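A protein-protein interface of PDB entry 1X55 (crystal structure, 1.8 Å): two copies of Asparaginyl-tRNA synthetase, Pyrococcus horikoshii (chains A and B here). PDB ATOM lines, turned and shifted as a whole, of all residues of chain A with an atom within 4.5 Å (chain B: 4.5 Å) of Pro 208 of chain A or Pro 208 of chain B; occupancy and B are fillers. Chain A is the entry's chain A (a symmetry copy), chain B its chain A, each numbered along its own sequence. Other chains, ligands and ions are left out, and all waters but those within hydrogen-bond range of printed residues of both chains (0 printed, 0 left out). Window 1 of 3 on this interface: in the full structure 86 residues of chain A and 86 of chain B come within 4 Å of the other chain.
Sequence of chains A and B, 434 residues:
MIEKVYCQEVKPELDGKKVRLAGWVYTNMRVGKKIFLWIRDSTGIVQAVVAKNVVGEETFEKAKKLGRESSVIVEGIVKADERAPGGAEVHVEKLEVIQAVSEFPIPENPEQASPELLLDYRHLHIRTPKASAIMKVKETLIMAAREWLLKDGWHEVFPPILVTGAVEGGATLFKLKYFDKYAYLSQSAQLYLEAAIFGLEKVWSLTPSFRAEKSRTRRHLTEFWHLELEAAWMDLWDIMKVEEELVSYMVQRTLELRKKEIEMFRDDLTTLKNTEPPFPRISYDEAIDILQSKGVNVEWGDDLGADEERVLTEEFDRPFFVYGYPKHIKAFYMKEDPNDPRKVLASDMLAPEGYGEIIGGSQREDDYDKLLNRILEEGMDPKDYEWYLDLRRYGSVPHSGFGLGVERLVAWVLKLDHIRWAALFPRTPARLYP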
ATOM      1  N   ILE A 161      14.309 -20.287 -25.130  1.00  0.00           N
ATOM      2  CA  ILE A 161      13.240 -21.098 -25.690  1.00  0.00           C
ATOM      3  C   ILE A 161      11.918 -20.351 -25.608  1.00  0.00           C
ATOM      4  O   ILE A 161      11.139 -20.396 -26.559  1.00  0.00           O
ATOM      5  CB  ILE A 161      13.165 -22.508 -25.002  1.00  0.00           C
ATOM      6  CG1 ILE A 161      14.527 -23.245 -25.096  1.00  0.00           C
ATOM      7  CG2 ILE A 161      12.008 -23.347 -25.596  1.00  0.00           C
ATOM      8  CD1 ILE A 161      15.097 -23.380 -26.475  1.00  0.00           C
ATOM      9  N   SER A 186      10.078 -21.320 -28.924  1.00  0.00           N
ATOM     10  CA  SER A 186      10.994 -21.068 -30.036  1.00  0.00           C
ATOM     11  C   SER A 186      10.929 -22.124 -31.146  1.00  0.00           C
ATOM     12  O   SER A 186      11.107 -23.318 -30.909  1.00  0.00           O
ATOM     13  CB  SER A 186      12.436 -20.945 -29.555  1.00  0.00           C
ATOM     14  OG  SER A 186      13.303 -20.752 -30.675  1.00  0.00           O
ATOM     15  N   THR A 207      19.578 -26.705 -29.589  1.00  0.00           N
ATOM     16  CA  THR A 207      18.397 -26.471 -28.737  1.00  0.00           C
ATOM     17  C   THR A 207      17.228 -27.292 -29.262  1.00  0.00           C
ATOM     18  O   THR A 207      17.207 -27.652 -30.468  1.00  0.00           O
ATOM     19  CB  THR A 207      17.963 -24.969 -28.730  1.00  0.00           C
ATOM     20  OG1 THR A 207      17.634 -24.558 -30.064  1.00  0.00           O
ATOM     21  CG2 THR A 207      19.134 -24.005 -28.256  1.00  0.00           C
ATOM     22  N   PRO A 208      16.251 -27.584 -28.403  1.00  0.00           N
ATOM     23  CA  PRO A 208      15.015 -28.142 -28.906  1.00  0.00           C
ATOM     24  C   PRO A 208      14.245 -26.984 -29.564  1.00  0.00           C
ATOM     25  O   PRO A 208      14.145 -25.886 -28.994  1.00  0.00           O
ATOM     26  CB  PRO A 208      14.303 -28.669 -27.652  1.00  0.00           C
ATOM     27  CG  PRO A 208      14.839 -27.805 -26.486  1.00  0.00           C
ATOM     28  CD  PRO A 208      16.234 -27.364 -26.928  1.00  0.00           C
ATOM     29  N   SER A 209      13.761 -27.230 -30.777  1.00  0.00           N
ATOM     30  CA  SER A 209      12.872 -26.292 -31.468  1.00  0.00           C
ATOM     31  C   SER A 209      11.469 -26.901 -31.566  1.00  0.00           C
ATOM     32  O   SER A 209      11.340 -28.122 -31.594  1.00  0.00           O
ATOM     33  CB  SER A 209      13.427 -25.997 -32.868  1.00  0.00           C
ATOM     34  OG  SER A 209      14.543 -25.159 -32.781  1.00  0.00           O
ATOM     35  N   PHE A 210      10.443 -26.043 -31.635  1.00  0.00           N
ATOM     36  CA  PHE A 210       9.045 -26.458 -31.484  1.00  0.00           C
ATOM     37  C   PHE A 210       8.257 -26.007 -32.679  1.00  0.00           C
ATOM     38  O   PHE A 210       8.299 -24.826 -33.038  1.00  0.00           O
ATOM     39  CB  PHE A 210       8.473 -25.907 -30.173  1.00  0.00           C
ATOM     40  CG  PHE A 210       9.202 -26.423 -28.972  1.00  0.00           C
ATOM     41  CD1 PHE A 210       8.784 -27.608 -28.354  1.00  0.00           C
ATOM     42  CD2 PHE A 210      10.367 -25.772 -28.512  1.00  0.00           C
ATOM     43  CE1 PHE A 210       9.522 -28.149 -27.248  1.00  0.00           C
ATOM     44  CE2 PHE A 210      11.085 -26.269 -27.415  1.00  0.00           C
ATOM     45  CZ  PHE A 210      10.659 -27.455 -26.773  1.00  0.00           C
ATOM     46  N   PHE A 224      12.018 -30.993 -32.030  1.00  0.00           N
ATOM     47  CA  PHE A 224      13.199 -31.600 -32.655  1.00  0.00           C
ATOM     48  C   PHE A 224      14.470 -30.891 -32.213  1.00  0.00           C
ATOM     49  O   PHE A 224      14.395 -29.789 -31.700  1.00  0.00           O
ATOM     50  CB  PHE A 224      13.067 -31.647 -34.196  1.00  0.00           C
ATOM     51  CG  PHE A 224      13.273 -30.308 -34.879  1.00  0.00           C
ATOM     52  CD1 PHE A 224      14.534 -29.925 -35.302  1.00  0.00           C
ATOM     53  CD2 PHE A 224      12.207 -29.425 -35.076  1.00  0.00           C
ATOM     54  CE1 PHE A 224      14.723 -28.677 -35.948  1.00  0.00           C
ATOM     55  CE2 PHE A 224      12.407 -28.176 -35.711  1.00  0.00           C
ATOM     56  CZ  PHE A 224      13.665 -27.832 -36.168  1.00  0.00           C
ATOM     57  N   TRP A 225      15.628 -31.532 -32.403  1.00  0.00           N
ATOM     58  CA  TRP A 225      16.869 -30.939 -31.949  1.00  0.00           C
ATOM     59  C   TRP A 225      17.514 -30.227 -33.136  1.00  0.00           C
ATOM     60  O   TRP A 225      17.664 -30.811 -34.218  1.00  0.00           O
ATOM     61  CB  TRP A 225      17.771 -31.997 -31.314  1.00  0.00           C
ATOM     62  CG  TRP A 225      17.322 -32.248 -29.910  1.00  0.00           C
ATOM     63  CD1 TRP A 225      16.289 -33.065 -29.504  1.00  0.00           C
ATOM     64  CD2 TRP A 225      17.766 -31.550 -28.743  1.00  0.00           C
ATOM     65  NE1 TRP A 225      16.086 -32.931 -28.145  1.00  0.00           N
ATOM     66  CE2 TRP A 225      16.993 -32.029 -27.647  1.00  0.00           C
ATOM     67  CE3 TRP A 225      18.752 -30.573 -28.502  1.00  0.00           C
ATOM     68  CZ2 TRP A 225      17.189 -31.578 -26.333  1.00  0.00           C
ATOM     69  CZ3 TRP A 225      18.950 -30.124 -27.167  1.00  0.00           C
ATOM     70  CH2 TRP A 225      18.163 -30.638 -26.116  1.00  0.00           C
ATOM     71  N   ILE B 161      11.058 -32.346 -24.085  1.00  0.00           N
ATOM     72  CA  ILE B 161      10.696 -31.134 -23.366  1.00  0.00           C
ATOM     73  C   ILE B 161       9.193 -31.094 -23.134  1.00  0.00           C
ATOM     74  O   ILE B 161       8.760 -30.710 -22.048  1.00  0.00           O
ATOM     75  CB  ILE B 161      11.215 -29.849 -24.103  1.00  0.00           C
ATOM     76  CG1 ILE B 161      12.748 -29.920 -24.330  1.00  0.00           C
ATOM     77  CG2 ILE B 161      10.800 -28.571 -23.334  1.00  0.00           C
ATOM     78  CD1 ILE B 161      13.574 -30.175 -23.106  1.00  0.00           C
ATOM     79  N   SER B 186       8.830 -29.509 -19.574  1.00  0.00           N
ATOM     80  CA  SER B 186       9.691 -30.258 -18.659  1.00  0.00           C
ATOM     81  C   SER B 186      10.404 -29.382 -17.621  1.00  0.00           C
ATOM     82  O   SER B 186      11.116 -28.436 -17.957  1.00  0.00           O
ATOM     83  CB  SER B 186      10.734 -31.074 -19.416  1.00  0.00           C
ATOM     84  OG  SER B 186      11.587 -31.747 -18.486  1.00  0.00           O
ATOM     85  N   THR B 207      19.650 -29.797 -21.165  1.00  0.00           N
ATOM     86  CA  THR B 207      18.371 -29.344 -21.743  1.00  0.00           C
ATOM     87  C   THR B 207      17.923 -28.072 -21.039  1.00  0.00           C
ATOM     88  O   THR B 207      18.336 -27.821 -19.876  1.00  0.00           O
ATOM     89  CB  THR B 207      17.238 -30.409 -21.576  1.00  0.00           C
ATOM     90  OG1 THR B 207      17.025 -30.669 -20.182  1.00  0.00           O
ATOM     91  CG2 THR B 207      17.625 -31.808 -22.223  1.00  0.00           C
ATOM     92  N   PRO B 208      17.082 -27.272 -21.696  1.00  0.00           N
ATOM     93  CA  PRO B 208      16.439 -26.190 -20.984  1.00  0.00           C
ATOM     94  C   PRO B 208      15.338 -26.825 -20.119  1.00  0.00           C
ATOM     95  O   PRO B 208      14.576 -27.683 -20.593  1.00  0.00           O
ATOM     96  CB  PRO B 208      15.860 -25.303 -22.095  1.00  0.00           C
ATOM     97  CG  PRO B 208      15.627 -26.251 -23.295  1.00  0.00           C
ATOM     98  CD  PRO B 208      16.655 -27.368 -23.122  1.00  0.00           C
ATOM     99  N   SER B 209      15.307 -26.436 -18.848  1.00  0.00           N
ATOM    100  CA  SER B 209      14.226 -26.823 -17.939  1.00  0.00           C
ATOM    101  C   SER B 209      13.386 -25.589 -17.592  1.00  0.00           C
ATOM    102  O   SER B 209      13.910 -24.478 -17.607  1.00  0.00           O
ATOM    103  CB  SER B 209      14.822 -27.440 -16.667  1.00  0.00           C
ATOM    104  OG  SER B 209      15.306 -28.725 -16.931  1.00  0.00           O
ATOM    105  N   PHE B 210      12.105 -25.802 -17.267  1.00  0.00           N
ATOM    106  CA  PHE B 210      11.120 -24.722 -17.153  1.00  0.00           C
ATOM    107  C   PHE B 210      10.475 -24.773 -15.799  1.00  0.00           C
ATOM    108  O   PHE B 210       9.979 -25.827 -15.390  1.00  0.00           O
ATOM    109  CB  PHE B 210      10.094 -24.826 -18.287  1.00  0.00           C
ATOM    110  CG  PHE B 210      10.722 -24.690 -19.638  1.00  0.00           C
ATOM    111  CD1 PHE B 210      10.854 -23.425 -20.225  1.00  0.00           C
ATOM    112  CD2 PHE B 210      11.267 -25.818 -20.289  1.00  0.00           C
ATOM    113  CE1 PHE B 210      11.522 -23.277 -21.487  1.00  0.00           C
ATOM    114  CE2 PHE B 210      11.897 -25.697 -21.535  1.00  0.00           C
ATOM    115  CZ  PHE B 210      12.018 -24.427 -22.143  1.00  0.00           C
ATOM    116  N   PHE B 224      16.034 -22.389 -17.483  1.00  0.00           N
ATOM    117  CA  PHE B 224      17.458 -22.509 -17.147  1.00  0.00           C
ATOM    118  C   PHE B 224      18.066 -23.743 -17.798  1.00  0.00           C
ATOM    119  O   PHE B 224      17.334 -24.620 -18.220  1.00  0.00           O
ATOM    120  CB  PHE B 224      17.686 -22.490 -15.616  1.00  0.00           C
ATOM    121  CG  PHE B 224      17.311 -23.781 -14.915  1.00  0.00           C
ATOM    122  CD1 PHE B 224      18.253 -24.779 -14.736  1.00  0.00           C
ATOM    123  CD2 PHE B 224      16.010 -24.003 -14.455  1.00  0.00           C
ATOM    124  CE1 PHE B 224      17.903 -25.982 -14.072  1.00  0.00           C
ATOM    125  CE2 PHE B 224      15.666 -25.212 -13.804  1.00  0.00           C
ATOM    126  CZ  PHE B 224      16.632 -26.177 -13.593  1.00  0.00           C
ATOM    127  N   TRP B 225      19.398 -23.798 -17.884  1.00  0.00           N
ATOM    128  CA  TRP B 225      20.038 -24.915 -18.546  1.00  0.00           C
ATOM    129  C   TRP B 225      20.454 -25.924 -17.477  1.00  0.00           C
ATOM    130  O   TRP B 225      21.099 -25.561 -16.483  1.00  0.00           O
ATOM    131  CB  TRP B 225      21.203 -24.435 -19.410  1.00  0.00           C
ATOM    132  CG  TRP B 225      20.671 -23.910 -20.705  1.00  0.00           C
ATOM    133  CD1 TRP B 225      20.145 -22.658 -20.939  1.00  0.00           C
ATOM    134  CD2 TRP B 225      20.447 -24.669 -21.897  1.00  0.00           C
ATOM    135  NE1 TRP B 225      19.631 -22.591 -22.218  1.00  0.00           N
ATOM    136  CE2 TRP B 225      19.824 -23.800 -22.839  1.00  0.00           C
ATOM    137  CE3 TRP B 225      20.720 -25.997 -22.278  1.00  0.00           C
ATOM    138  CZ2 TRP B 225      19.489 -24.213 -24.137  1.00  0.00           C
ATOM    139  CZ3 TRP B 225      20.384 -26.407 -23.598  1.00  0.00           C
ATOM    140  CH2 TRP B 225      19.777 -25.504 -24.494  1.00  0.00           C
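The backbone carbonyl oxygen (O) of Ile 161 of chain B lies within hydrogen-bond range of the backbone NH (N) of Ser 186 of chain B, 2.8 Å away.
O of Ser 186 of chain B sits at hydrogen-bond distance from N of Phe 210 of chain B (2.9 Å).
The backbone carbonyl oxygen (O) of Ile 161 of chain A sits at hydrogen-bond distance from the backbone NH (N) of Ser 186 of chain A (2.8 Å).
The backbone carbonyl oxygen (O) of Ser 186 of chain A sits at hydrogen-bond distance from the backbone NH (N) of Phe 210 of chain A (2.9 Å).
Among the printed residues, pairs that only touch across the chains: Ile 161 of chain A with Phe 210 of chain B (3.6 Å), Phe 210 of chain A with Ile 161 of chain B (3.6 Å), Pro 208 of chain A with Pro 208 of chain B (3.6 Å), Ile 161 of chain A with Pro 208 of chain B (3.7 Å) and Pro 208 of chain A with Ile 161 of chain B (3.7 Å).
Pro 208 of chain A touches just these residues of chain B: Ile 161 (3.7 Å) and Pro 208 (3.6 Å).
Of the printed residues of chain A, Ile 161 of chain B touches Pro 208 and Phe 210.
Of the printed residues of chain A, Phe 210 of chain B touches Ile 161.
Of the printed residues of chain B, Ile 161 of chain A touches Pro 208 and Phe 210.
Printed residues of chain B within 4 Å of Phe 210 of chain A: Ile 161 (3.6 Å).
The nearest printed residue of chain B that does not touch Pro 208 of chain A is Trp 225 of chain B (4.7 Å).
The nearest printed residue of chain A that does not touch Pro 208 of chain B is Trp 225 of chain A (4.7 Å).
Of the 8 printed residues of chain B, 3 touch a printed residue of chain A.
Hydrophobic or aromatic side chains of chain B within 4 Å of the printed part of chain A: Ile 161, Pro 208 and Phe 210.
Of the 8 printed residues of chain A, 3 touch a printed residue of chain B.
Hydrophobic or aromatic side chains of chain A that line the printed part of chain B: Ile 161, Pro 208 and Phe 210.
Among the printed residues, 5 pairs touch across the chains.
Ile 161 of chain A touches Pro 208 of chain B, and with the chains exchanged Pro 208 of chain A touches Ile 161 of chain B.
Ile 161 of chain A touches Phe 210 of chain B, and with the chains exchanged Phe 210 of chain A touches Ile 161 of chain B.
Pro 208 of chain A touches its own counterpart, Pro 208 of chain B.
Positions printed for both chains: 161, 186, 207, 208, 209, 210, 224 and 225.
Of the 5 pairs that touch across the chains among the printed residues, 5 have their exchanged pair printed and touching as well.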
